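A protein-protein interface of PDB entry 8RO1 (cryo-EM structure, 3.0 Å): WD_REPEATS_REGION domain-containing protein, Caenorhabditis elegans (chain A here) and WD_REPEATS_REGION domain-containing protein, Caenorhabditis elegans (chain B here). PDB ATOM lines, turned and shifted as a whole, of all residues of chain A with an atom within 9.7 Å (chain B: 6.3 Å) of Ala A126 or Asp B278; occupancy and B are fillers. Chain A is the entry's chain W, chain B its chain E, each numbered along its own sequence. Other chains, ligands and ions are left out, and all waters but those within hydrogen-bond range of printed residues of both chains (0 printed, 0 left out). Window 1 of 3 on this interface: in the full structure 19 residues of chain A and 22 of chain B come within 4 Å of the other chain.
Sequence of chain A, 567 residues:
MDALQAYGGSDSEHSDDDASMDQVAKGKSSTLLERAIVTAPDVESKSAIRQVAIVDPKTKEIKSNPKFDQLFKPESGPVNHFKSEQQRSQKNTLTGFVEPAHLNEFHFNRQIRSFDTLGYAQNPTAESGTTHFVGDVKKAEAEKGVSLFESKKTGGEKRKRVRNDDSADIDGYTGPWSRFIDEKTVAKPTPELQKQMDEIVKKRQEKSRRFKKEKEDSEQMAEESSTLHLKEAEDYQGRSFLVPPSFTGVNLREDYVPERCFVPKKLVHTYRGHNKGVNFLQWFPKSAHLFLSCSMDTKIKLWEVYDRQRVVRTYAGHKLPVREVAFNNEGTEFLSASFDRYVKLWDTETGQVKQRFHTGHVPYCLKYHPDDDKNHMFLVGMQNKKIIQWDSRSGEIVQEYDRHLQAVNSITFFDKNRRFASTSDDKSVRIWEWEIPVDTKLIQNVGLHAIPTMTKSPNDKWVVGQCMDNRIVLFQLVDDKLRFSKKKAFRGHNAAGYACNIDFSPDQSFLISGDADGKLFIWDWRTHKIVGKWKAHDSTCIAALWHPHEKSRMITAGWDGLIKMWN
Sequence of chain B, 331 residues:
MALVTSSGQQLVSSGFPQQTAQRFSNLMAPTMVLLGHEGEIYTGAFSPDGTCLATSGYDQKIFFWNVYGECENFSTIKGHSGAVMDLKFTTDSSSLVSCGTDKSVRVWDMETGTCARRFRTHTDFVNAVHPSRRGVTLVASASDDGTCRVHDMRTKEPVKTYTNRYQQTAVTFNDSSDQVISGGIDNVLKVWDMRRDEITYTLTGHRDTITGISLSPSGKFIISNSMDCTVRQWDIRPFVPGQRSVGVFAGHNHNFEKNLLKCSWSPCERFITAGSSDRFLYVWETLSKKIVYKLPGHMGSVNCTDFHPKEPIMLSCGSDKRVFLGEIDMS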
ATOM      1  N   PHE A  68     -16.105 -38.783  20.049  1.00  0.00           N
ATOM      2  CA  PHE A  68     -16.239 -37.539  20.794  1.00  0.00           C
ATOM      3  C   PHE A  68     -16.925 -37.765  22.129  1.00  0.00           C
ATOM      4  O   PHE A  68     -16.455 -37.306  23.174  1.00  0.00           O
ATOM      5  CB  PHE A  68     -17.035 -36.524  19.986  1.00  0.00           C
ATOM      6  CG  PHE A  68     -17.379 -35.287  20.750  1.00  0.00           C
ATOM      7  CD1 PHE A  68     -16.413 -34.362  21.043  1.00  0.00           C
ATOM      8  CD2 PHE A  68     -18.659 -35.060  21.196  1.00  0.00           C
ATOM      9  CE1 PHE A  68     -16.713 -33.223  21.742  1.00  0.00           C
ATOM     10  CE2 PHE A  68     -18.965 -33.925  21.906  1.00  0.00           C
ATOM     11  CZ  PHE A  68     -17.988 -33.001  22.176  1.00  0.00           C
ATOM     12  N   PHE A  72     -14.322 -37.067  25.010  1.00  0.00           N
ATOM     13  CA  PHE A  72     -14.550 -35.825  25.738  1.00  0.00           C
ATOM     14  C   PHE A  72     -15.406 -35.973  26.981  1.00  0.00           C
ATOM     15  O   PHE A  72     -15.297 -35.111  27.859  1.00  0.00           O
ATOM     16  CB  PHE A  72     -15.039 -34.743  24.787  1.00  0.00           C
ATOM     17  CG  PHE A  72     -13.932 -34.219  23.922  1.00  0.00           C
ATOM     18  CD1 PHE A  72     -13.444 -34.951  22.863  1.00  0.00           C
ATOM     19  CD2 PHE A  72     -13.315 -33.029  24.242  1.00  0.00           C
ATOM     20  CE1 PHE A  72     -12.372 -34.507  22.139  1.00  0.00           C
ATOM     21  CE2 PHE A  72     -12.264 -32.563  23.504  1.00  0.00           C
ATOM     22  CZ  PHE A  72     -11.777 -33.308  22.459  1.00  0.00           C
ATOM     23  N   GLU A  99       3.101 -27.877  25.407  1.00  0.00           N
ATOM     24  CA  GLU A  99       3.000 -28.582  24.140  1.00  0.00           C
ATOM     25  C   GLU A  99       3.570 -27.699  23.042  1.00  0.00           C
ATOM     26  O   GLU A  99       3.385 -26.479  23.081  1.00  0.00           O
ATOM     27  CB  GLU A  99       1.547 -28.932  23.794  1.00  0.00           C
ATOM     28  CG  GLU A  99       0.648 -27.732  23.620  1.00  0.00           C
ATOM     29  CD  GLU A  99      -0.798 -28.107  23.560  1.00  0.00           C
ATOM     30  OE1 GLU A  99      -1.098 -29.246  23.158  1.00  0.00           O
ATOM     31  OE2 GLU A  99      -1.642 -27.260  23.914  1.00  0.00           O
ATOM     32  N   HIS A 102       2.905 -24.078  16.461  1.00  0.00           N
ATOM     33  CA  HIS A 102       3.372 -23.377  15.280  1.00  0.00           C
ATOM     34  C   HIS A 102       2.380 -22.286  14.958  1.00  0.00           C
ATOM     35  O   HIS A 102       1.172 -22.507  15.061  1.00  0.00           O
ATOM     36  CB  HIS A 102       3.465 -24.277  14.062  1.00  0.00           C
ATOM     37  CG  HIS A 102       4.362 -25.462  14.218  1.00  0.00           C
ATOM     38  ND1 HIS A 102       3.944 -26.638  14.798  1.00  0.00           N
ATOM     39  CD2 HIS A 102       5.629 -25.680  13.799  1.00  0.00           C
ATOM     40  CE1 HIS A 102       4.928 -27.517  14.763  1.00  0.00           C
ATOM     41  NE2 HIS A 102       5.962 -26.960  14.164  1.00  0.00           N
ATOM     42  N   LEU A 103       2.881 -21.114  14.562  1.00  0.00           N
ATOM     43  CA  LEU A 103       1.979 -20.047  14.184  1.00  0.00           C
ATOM     44  C   LEU A 103       2.537 -19.274  13.002  1.00  0.00           C
ATOM     45  O   LEU A 103       3.652 -19.517  12.535  1.00  0.00           O
ATOM     46  CB  LEU A 103       1.814 -19.090  15.361  1.00  0.00           C
ATOM     47  CG  LEU A 103       1.118 -19.536  16.630  1.00  0.00           C
ATOM     48  CD1 LEU A 103       1.244 -18.392  17.600  1.00  0.00           C
ATOM     49  CD2 LEU A 103      -0.324 -19.880  16.400  1.00  0.00           C
ATOM     50  N   GLN A 122      -5.429  -9.891  20.861  1.00  0.00           N
ATOM     51  CA  GLN A 122      -6.482 -10.815  20.500  1.00  0.00           C
ATOM     52  C   GLN A 122      -6.116 -12.182  21.053  1.00  0.00           C
ATOM     53  O   GLN A 122      -4.980 -12.639  20.907  1.00  0.00           O
ATOM     54  CB  GLN A 122      -6.634 -10.850  18.983  1.00  0.00           C
ATOM     55  CG  GLN A 122      -7.863 -11.571  18.511  1.00  0.00           C
ATOM     56  CD  GLN A 122      -7.986 -11.586  17.007  1.00  0.00           C
ATOM     57  OE1 GLN A 122      -7.556 -10.655  16.332  1.00  0.00           O
ATOM     58  NE2 GLN A 122      -8.650 -12.606  16.480  1.00  0.00           N
ATOM     59  N   ASN A 123      -7.078 -12.808  21.712  1.00  0.00           N
ATOM     60  CA  ASN A 123      -6.830 -13.809  22.741  1.00  0.00           C
ATOM     61  C   ASN A 123      -6.140 -15.052  22.181  1.00  0.00           C
ATOM     62  O   ASN A 123      -6.692 -15.681  21.270  1.00  0.00           O
ATOM     63  CB  ASN A 123      -8.168 -14.201  23.361  1.00  0.00           C
ATOM     64  CG  ASN A 123      -8.022 -15.020  24.622  1.00  0.00           C
ATOM     65  OD1 ASN A 123      -6.929 -15.392  25.015  1.00  0.00           O
ATOM     66  ND2 ASN A 123      -9.142 -15.311  25.258  1.00  0.00           N
ATOM     67  N   PRO A 124      -4.966 -15.458  22.686  1.00  0.00           N
ATOM     68  CA  PRO A 124      -4.239 -16.533  22.011  1.00  0.00           C
ATOM     69  C   PRO A 124      -4.889 -17.879  22.158  1.00  0.00           C
ATOM     70  O   PRO A 124      -4.546 -18.785  21.392  1.00  0.00           O
ATOM     71  CB  PRO A 124      -2.859 -16.522  22.671  1.00  0.00           C
ATOM     72  CG  PRO A 124      -3.008 -15.838  23.878  1.00  0.00           C
ATOM     73  CD  PRO A 124      -4.125 -14.875  23.738  1.00  0.00           C
ATOM     74  N   THR A 125      -5.780 -18.067  23.123  1.00  0.00           N
ATOM     75  CA  THR A 125      -6.103 -19.413  23.552  1.00  0.00           C
ATOM     76  C   THR A 125      -6.937 -20.111  22.492  1.00  0.00           C
ATOM     77  O   THR A 125      -7.752 -19.496  21.805  1.00  0.00           O
ATOM     78  CB  THR A 125      -6.918 -19.389  24.837  1.00  0.00           C
ATOM     79  OG1 THR A 125      -8.077 -18.574  24.655  1.00  0.00           O
ATOM     80  CG2 THR A 125      -6.131 -18.798  25.929  1.00  0.00           C
ATOM     81  N   ALA A 126      -6.744 -21.419  22.385  1.00  0.00           N
ATOM     82  CA  ALA A 126      -7.737 -22.259  21.749  1.00  0.00           C
ATOM     83  C   ALA A 126      -9.033 -22.222  22.541  1.00  0.00           C
ATOM     84  O   ALA A 126      -9.033 -22.113  23.769  1.00  0.00           O
ATOM     85  CB  ALA A 126      -7.215 -23.686  21.642  1.00  0.00           C
ATOM     86  N   GLU A 127     -10.149 -22.333  21.826  1.00  0.00           N
ATOM     87  CA  GLU A 127     -11.472 -22.369  22.441  1.00  0.00           C
ATOM     88  C   GLU A 127     -11.741 -21.121  23.278  1.00  0.00           C
ATOM     89  O   GLU A 127     -12.237 -21.197  24.401  1.00  0.00           O
ATOM     90  CB  GLU A 127     -11.622 -23.639  23.277  1.00  0.00           C
ATOM     91  CG  GLU A 127     -11.250 -24.885  22.487  1.00  0.00           C
ATOM     92  CD  GLU A 127     -11.727 -26.166  23.127  1.00  0.00           C
ATOM     93  OE1 GLU A 127     -12.935 -26.278  23.424  1.00  0.00           O
ATOM     94  OE2 GLU A 127     -10.889 -27.071  23.320  1.00  0.00           O
ATOM     95  N   SER A 128     -11.397 -19.960  22.722  1.00  0.00           N
ATOM     96  CA  SER A 128     -11.430 -18.700  23.455  1.00  0.00           C
ATOM     97  C   SER A 128     -12.842 -18.285  23.852  1.00  0.00           C
ATOM     98  O   SER A 128     -12.996 -17.437  24.736  1.00  0.00           O
ATOM     99  CB  SER A 128     -10.805 -17.584  22.626  1.00  0.00           C
ATOM    100  OG  SER A 128     -11.499 -17.416  21.405  1.00  0.00           O
ATOM    101  N   GLY A 129     -13.867 -18.876  23.244  1.00  0.00           N
ATOM    102  CA  GLY A 129     -15.239 -18.537  23.575  1.00  0.00           C
ATOM    103  C   GLY A 129     -15.548 -17.088  23.259  1.00  0.00           C
ATOM    104  O   GLY A 129     -15.124 -16.550  22.230  1.00  0.00           O
ATOM    105  N   THR A 130     -16.311 -16.440  24.138  1.00  0.00           N
ATOM    106  CA  THR A 130     -16.581 -15.017  23.972  1.00  0.00           C
ATOM    107  C   THR A 130     -15.369 -14.126  24.211  1.00  0.00           C
ATOM    108  O   THR A 130     -15.370 -12.982  23.745  1.00  0.00           O
ATOM    109  CB  THR A 130     -17.727 -14.584  24.893  1.00  0.00           C
ATOM    110  OG1 THR A 130     -18.101 -13.238  24.580  1.00  0.00           O
ATOM    111  CG2 THR A 130     -17.332 -14.656  26.370  1.00  0.00           C
ATOM    112  N   THR A 131     -14.336 -14.603  24.906  1.00  0.00           N
ATOM    113  CA  THR A 131     -13.201 -13.746  25.255  1.00  0.00           C
ATOM    114  C   THR A 131     -12.255 -13.601  24.064  1.00  0.00           C
ATOM    115  O   THR A 131     -11.120 -14.080  24.053  1.00  0.00           O
ATOM    116  CB  THR A 131     -12.474 -14.290  26.472  1.00  0.00           C
ATOM    117  OG1 THR A 131     -13.430 -14.778  27.417  1.00  0.00           O
ATOM    118  CG2 THR A 131     -11.651 -13.190  27.114  1.00  0.00           C
ATOM    119  N   GLY B 251     -18.267 -24.683  17.428  1.00  0.00           N
ATOM    120  CA  GLY B 251     -17.361 -25.496  18.209  1.00  0.00           C
ATOM    121  C   GLY B 251     -15.947 -25.258  17.750  1.00  0.00           C
ATOM    122  O   GLY B 251     -15.016 -25.226  18.557  1.00  0.00           O
ATOM    123  N   HIS B 252     -15.778 -25.085  16.447  1.00  0.00           N
ATOM    124  CA  HIS B 252     -14.493 -24.674  15.930  1.00  0.00           C
ATOM    125  C   HIS B 252     -14.231 -23.220  16.298  1.00  0.00           C
ATOM    126  O   HIS B 252     -15.088 -22.523  16.843  1.00  0.00           O
ATOM    127  CB  HIS B 252     -14.446 -24.931  14.434  1.00  0.00           C
ATOM    128  CG  HIS B 252     -15.300 -24.005  13.648  1.00  0.00           C
ATOM    129  ND1 HIS B 252     -16.641 -24.228  13.440  1.00  0.00           N
ATOM    130  CD2 HIS B 252     -14.999 -22.866  12.993  1.00  0.00           C
ATOM    131  CE1 HIS B 252     -17.136 -23.241  12.719  1.00  0.00           C
ATOM    132  NE2 HIS B 252     -16.159 -22.404  12.430  1.00  0.00           N
ATOM    133  N   ASN B 253     -13.021 -22.765  15.992  1.00  0.00           N
ATOM    134  CA  ASN B 253     -12.574 -21.429  16.349  1.00  0.00           C
ATOM    135  C   ASN B 253     -11.659 -20.861  15.276  1.00  0.00           C
ATOM    136  O   ASN B 253     -10.962 -21.612  14.593  1.00  0.00           O
ATOM    137  CB  ASN B 253     -11.841 -21.493  17.686  1.00  0.00           C
ATOM    138  CG  ASN B 253     -11.855 -20.186  18.429  1.00  0.00           C
ATOM    139  OD1 ASN B 253     -12.862 -19.485  18.469  1.00  0.00           O
ATOM    140  ND2 ASN B 253     -10.725 -19.851  19.035  1.00  0.00           N
ATOM    141  N   HIS B 254     -11.680 -19.536  15.114  1.00  0.00           N
ATOM    142  CA  HIS B 254     -10.714 -18.844  14.268  1.00  0.00           C
ATOM    143  C   HIS B 254      -9.877 -17.927  15.150  1.00  0.00           C
ATOM    144  O   HIS B 254     -10.421 -17.047  15.822  1.00  0.00           O
ATOM    145  CB  HIS B 254     -11.421 -18.011  13.201  1.00  0.00           C
ATOM    146  CG  HIS B 254     -12.171 -18.814  12.188  1.00  0.00           C
ATOM    147  ND1 HIS B 254     -13.205 -19.655  12.524  1.00  0.00           N
ATOM    148  CD2 HIS B 254     -12.065 -18.867  10.841  1.00  0.00           C
ATOM    149  CE1 HIS B 254     -13.684 -20.219  11.433  1.00  0.00           C
ATOM    150  NE2 HIS B 254     -13.015 -19.753  10.396  1.00  0.00           N
ATOM    151  N   ASN B 255      -8.557 -18.112  15.116  1.00  0.00           N
ATOM    152  CA  ASN B 255      -7.620 -17.347  15.931  1.00  0.00           C
ATOM    153  C   ASN B 255      -7.184 -16.043  15.262  1.00  0.00           C
ATOM    154  O   ASN B 255      -7.636 -15.677  14.179  1.00  0.00           O
ATOM    155  CB  ASN B 255      -6.425 -18.206  16.378  1.00  0.00           C
ATOM    156  CG  ASN B 255      -5.477 -18.671  15.246  1.00  0.00           C
ATOM    157  OD1 ASN B 255      -4.536 -19.399  15.552  1.00  0.00           O
ATOM    158  ND2 ASN B 255      -5.786 -18.418  13.976  1.00  0.00           N
ATOM    159  N   SER B 276     -10.105 -25.326  11.703  1.00  0.00           N
ATOM    160  CA  SER B 276     -10.266 -24.759  13.031  1.00  0.00           C
ATOM    161  C   SER B 276      -8.909 -24.328  13.556  1.00  0.00           C
ATOM    162  O   SER B 276      -7.918 -25.027  13.345  1.00  0.00           O
ATOM    163  CB  SER B 276     -10.902 -25.775  13.967  1.00  0.00           C
ATOM    164  OG  SER B 276     -11.244 -25.170  15.186  1.00  0.00           O
ATOM    165  N   SER B 277      -8.858 -23.189  14.232  1.00  0.00           N
ATOM    166  CA  SER B 277      -7.594 -22.752  14.809  1.00  0.00           C
ATOM    167  C   SER B 277      -7.222 -23.486  16.092  1.00  0.00           C
ATOM    168  O   SER B 277      -6.066 -23.399  16.516  1.00  0.00           O
ATOM    169  CB  SER B 277      -7.637 -21.267  15.122  1.00  0.00           C
ATOM    170  OG  SER B 277      -7.762 -20.508  13.939  1.00  0.00           O
ATOM    171  N   ASP B 278      -8.154 -24.199  16.723  1.00  0.00           N
ATOM    172  CA  ASP B 278      -7.895 -24.902  17.977  1.00  0.00           C
ATOM    173  C   ASP B 278      -7.200 -26.249  17.811  1.00  0.00           C
ATOM    174  O   ASP B 278      -7.223 -27.027  18.763  1.00  0.00           O
ATOM    175  CB  ASP B 278      -9.190 -25.060  18.777  1.00  0.00           C
ATOM    176  CG  ASP B 278     -10.204 -25.937  18.104  1.00  0.00           C
ATOM    177  OD1 ASP B 278      -9.952 -26.463  17.006  1.00  0.00           O
ATOM    178  OD2 ASP B 278     -11.283 -26.119  18.692  1.00  0.00           O
ATOM    179  N   ARG B 279      -6.631 -26.544  16.640  1.00  0.00           N
ATOM    180  CA  ARG B 279      -5.974 -27.802  16.272  1.00  0.00           C
ATOM    181  C   ARG B 279      -6.895 -29.003  16.070  1.00  0.00           C
ATOM    182  O   ARG B 279      -6.450 -30.024  15.542  1.00  0.00           O
ATOM    183  CB  ARG B 279      -4.969 -28.226  17.350  1.00  0.00           C
ATOM    184  CG  ARG B 279      -3.992 -27.179  17.802  1.00  0.00           C
ATOM    185  CD  ARG B 279      -3.216 -27.675  18.997  1.00  0.00           C
ATOM    186  NE  ARG B 279      -2.156 -26.733  19.344  1.00  0.00           N
ATOM    187  CZ  ARG B 279      -0.988 -27.039  19.900  1.00  0.00           C
ATOM    188  NH1 ARG B 279      -0.093 -26.075  20.087  1.00  0.00           N
ATOM    189  NH2 ARG B 279      -0.694 -28.272  20.286  1.00  0.00           N
ATOM    190  N   PHE B 280      -8.158 -28.917  16.470  1.00  0.00           N
ATOM    191  CA  PHE B 280      -9.049 -30.069  16.402  1.00  0.00           C
ATOM    192  C   PHE B 280      -9.676 -30.194  15.021  1.00  0.00           C
ATOM    193  O   PHE B 280     -10.079 -29.199  14.415  1.00  0.00           O
ATOM    194  CB  PHE B 280     -10.104 -30.012  17.501  1.00  0.00           C
ATOM    195  CG  PHE B 280      -9.524 -30.076  18.883  1.00  0.00           C
ATOM    196  CD1 PHE B 280      -8.968 -31.243  19.352  1.00  0.00           C
ATOM    197  CD2 PHE B 280      -9.607 -29.002  19.732  1.00  0.00           C
ATOM    198  CE1 PHE B 280      -8.455 -31.320  20.613  1.00  0.00           C
ATOM    199  CE2 PHE B 280      -9.094 -29.072  21.001  1.00  0.00           C
ATOM    200  CZ  PHE B 280      -8.517 -30.232  21.444  1.00  0.00           C
ATOM    201  N   LEU B 281      -9.725 -31.423  14.510  1.00  0.00           N
ATOM    202  CA  LEU B 281     -10.521 -31.747  13.329  1.00  0.00           C
ATOM    203  C   LEU B 281     -11.979 -31.911  13.720  1.00  0.00           C
ATOM    204  O   LEU B 281     -12.339 -32.897  14.369  1.00  0.00           O
ATOM    205  CB  LEU B 281     -10.047 -33.050  12.700  1.00  0.00           C
ATOM    206  CG  LEU B 281      -8.558 -33.204  12.451  1.00  0.00           C
ATOM    207  CD1 LEU B 281      -8.244 -34.519  11.733  1.00  0.00           C
ATOM    208  CD2 LEU B 281      -7.975 -32.029  11.767  1.00  0.00           C
ATOM    209  N   TYR B 282     -12.827 -30.975  13.320  1.00  0.00           N
ATOM    210  CA  TYR B 282     -14.242 -31.073  13.635  1.00  0.00           C
ATOM    211  C   TYR B 282     -14.970 -31.802  12.518  1.00  0.00           C
ATOM    212  O   TYR B 282     -14.644 -31.627  11.347  1.00  0.00           O
ATOM    213  CB  TYR B 282     -14.806 -29.674  13.804  1.00  0.00           C
ATOM    214  CG  TYR B 282     -14.468 -29.076  15.129  1.00  0.00           C
ATOM    215  CD1 TYR B 282     -15.281 -29.262  16.222  1.00  0.00           C
ATOM    216  CD2 TYR B 282     -13.317 -28.345  15.294  1.00  0.00           C
ATOM    217  CE1 TYR B 282     -14.973 -28.704  17.428  1.00  0.00           C
ATOM    218  CE2 TYR B 282     -12.993 -27.807  16.496  1.00  0.00           C
ATOM    219  CZ  TYR B 282     -13.820 -27.982  17.561  1.00  0.00           C
ATOM    220  OH  TYR B 282     -13.495 -27.428  18.771  1.00  0.00           O
ATOM    221  N   LYS B 294     -14.040 -35.195  17.135  1.00  0.00           N
ATOM    222  CA  LYS B 294     -13.194 -34.070  17.543  1.00  0.00           C
ATOM    223  C   LYS B 294     -11.806 -34.630  17.774  1.00  0.00           C
ATOM    224  O   LYS B 294     -11.485 -35.123  18.856  1.00  0.00           O
ATOM    225  CB  LYS B 294     -13.728 -33.396  18.790  1.00  0.00           C
ATOM    226  CG  LYS B 294     -13.163 -32.039  19.050  1.00  0.00           C
ATOM    227  CD  LYS B 294     -13.906 -31.398  20.183  1.00  0.00           C
ATOM    228  CE  LYS B 294     -13.192 -30.186  20.704  1.00  0.00           C
ATOM    229  NZ  LYS B 294     -13.834 -29.677  21.936  1.00  0.00           N
ATOM    230  N   GLY B 300      -1.112 -27.033  15.406  1.00  0.00           N
ATOM    231  CA  GLY B 300      -1.396 -25.669  15.034  1.00  0.00           C
ATOM    232  C   GLY B 300      -2.716 -25.575  14.300  1.00  0.00           C
ATOM    233  O   GLY B 300      -3.483 -26.536  14.238  1.00  0.00           O
ATOM    234  N   SER B 301      -2.969 -24.393  13.745  1.00  0.00           N
ATOM    235  CA  SER B 301      -4.198 -24.116  13.003  1.00  0.00           C
ATOM    236  C   SER B 301      -4.420 -25.083  11.850  1.00  0.00           C
ATOM    237  O   SER B 301      -3.597 -25.168  10.941  1.00  0.00           O
ATOM    238  CB  SER B 301      -4.153 -22.686  12.470  1.00  0.00           C
ATOM    239  OG  SER B 301      -4.192 -21.751  13.530  1.00  0.00           O
ATOM    240  N   VAL B 302      -5.538 -25.810  11.890  1.00  0.00           N
ATOM    241  CA  VAL B 302      -5.917 -26.748  10.832  1.00  0.00           C
ATOM    242  C   VAL B 302      -6.558 -25.954   9.699  1.00  0.00           C
ATOM    243  O   VAL B 302      -7.751 -25.658   9.737  1.00  0.00           O
ATOM    244  CB  VAL B 302      -6.853 -27.837  11.351  1.00  0.00           C
ATOM    245  CG1 VAL B 302      -7.186 -28.815  10.253  1.00  0.00           C
ATOM    246  CG2 VAL B 302      -6.185 -28.547  12.494  1.00  0.00           C
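The side-chain carboxylate of Glu A99 is in salt-bridge range of the guanidinium group of Arg B279.
The side-chain amino group (NZ) of Lys B294 lies within salt-bridge range of the side-chain carboxylate (OE1) of Glu A127 (3.8 Å).
The side-chain hydroxyl (OG) of Ser A128 is in hydrogen-bond range of the side-chain amide nitrogen (ND2) of Asn B253 (3.5 Å).
The backbone NH (N) of Asn B253 is in hydrogen-bond range of the side-chain hydroxyl (OG) of Ser B276 (3.1 Å).
The backbone carbonyl oxygen (O) of Asn B253 is in hydrogen-bond range of the backbone NH (N) of Ser B277 (2.7 Å).
The backbone NH (N) of Asn B255 lies within hydrogen-bond range of the side-chain hydroxyl (OG) of Ser B277 (2.8 Å).
The side-chain amide oxygen of Asn B255 sits at hydrogen-bond distance from the side-chain hydroxyl of Ser B301 (3.1 Å).
The side-chain hydroxyl (OG) of Ser B276 is in hydrogen-bond range of the side-chain carboxylate (OD1) of Asp B278.
The side-chain carboxylate (OD2) of Asp B278 sits at hydrogen-bond distance from the side-chain hydroxyl (OH) of Tyr B282.
Among the printed residues, merely in contact across the chains: Phe A68 with Lys B294, Phe A72 with Lys B294, Gln A122 with Asn B255, Ala A126 with Asp B278, Glu A127 with Asn B253, Glu A127 with Asp B278 and Glu A127 with Phe B280.
Ala A126 touches just one residue of chain B: Asp B278.
Printed residues of chain A within 4 Å of Asp B278: Ala A126 (3.7 Å) and Glu A127 (3.99 Å).
No residue of chain A comes within 4 Å of Ser B277.
Phe B280 touches just one residue of chain A: Glu A127.
Printed residues of chain A within 4 Å of Asn B255: Gln A122.
Of the printed residues of chain B, Glu A127 touches Asn B253 (3.8 Å), Asp B278 (3.99 Å), Phe B280 (3.6 Å) and Lys B294 (3.8 Å).
Of the printed residues of chain A, Asn B253 touches Glu A127 (3.8 Å) and Ser A128 (3.5 Å).
The nearest printed residue of chain B that does not touch Phe A68 is Tyr B282 (6.5 Å).
Of the 16 printed residues of chain B, 6 touch a printed residue of chain A.
Hydrophobic or aromatic side chains of chain B within 4 Å of the printed part of chain A: Phe B280.
Of the 15 printed residues of chain A, 7 touch a printed residue of chain B.
Hydrophobic or aromatic side chains of chain A that line the printed part of chain B: Phe A68, Phe A72 and Ala A126.
Along chain A the printed residues that touch a printed residue of chain B span positions 68 to 128.
Among the printed residues, 10 pairs touch across the chains.
Among the printed residues, Asp or Glu carboxylates within 4 Å of a Lys or Arg side-chain nitrogen of the other chain: Glu A99 with Arg B279 and Glu A127 with Lys B294.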
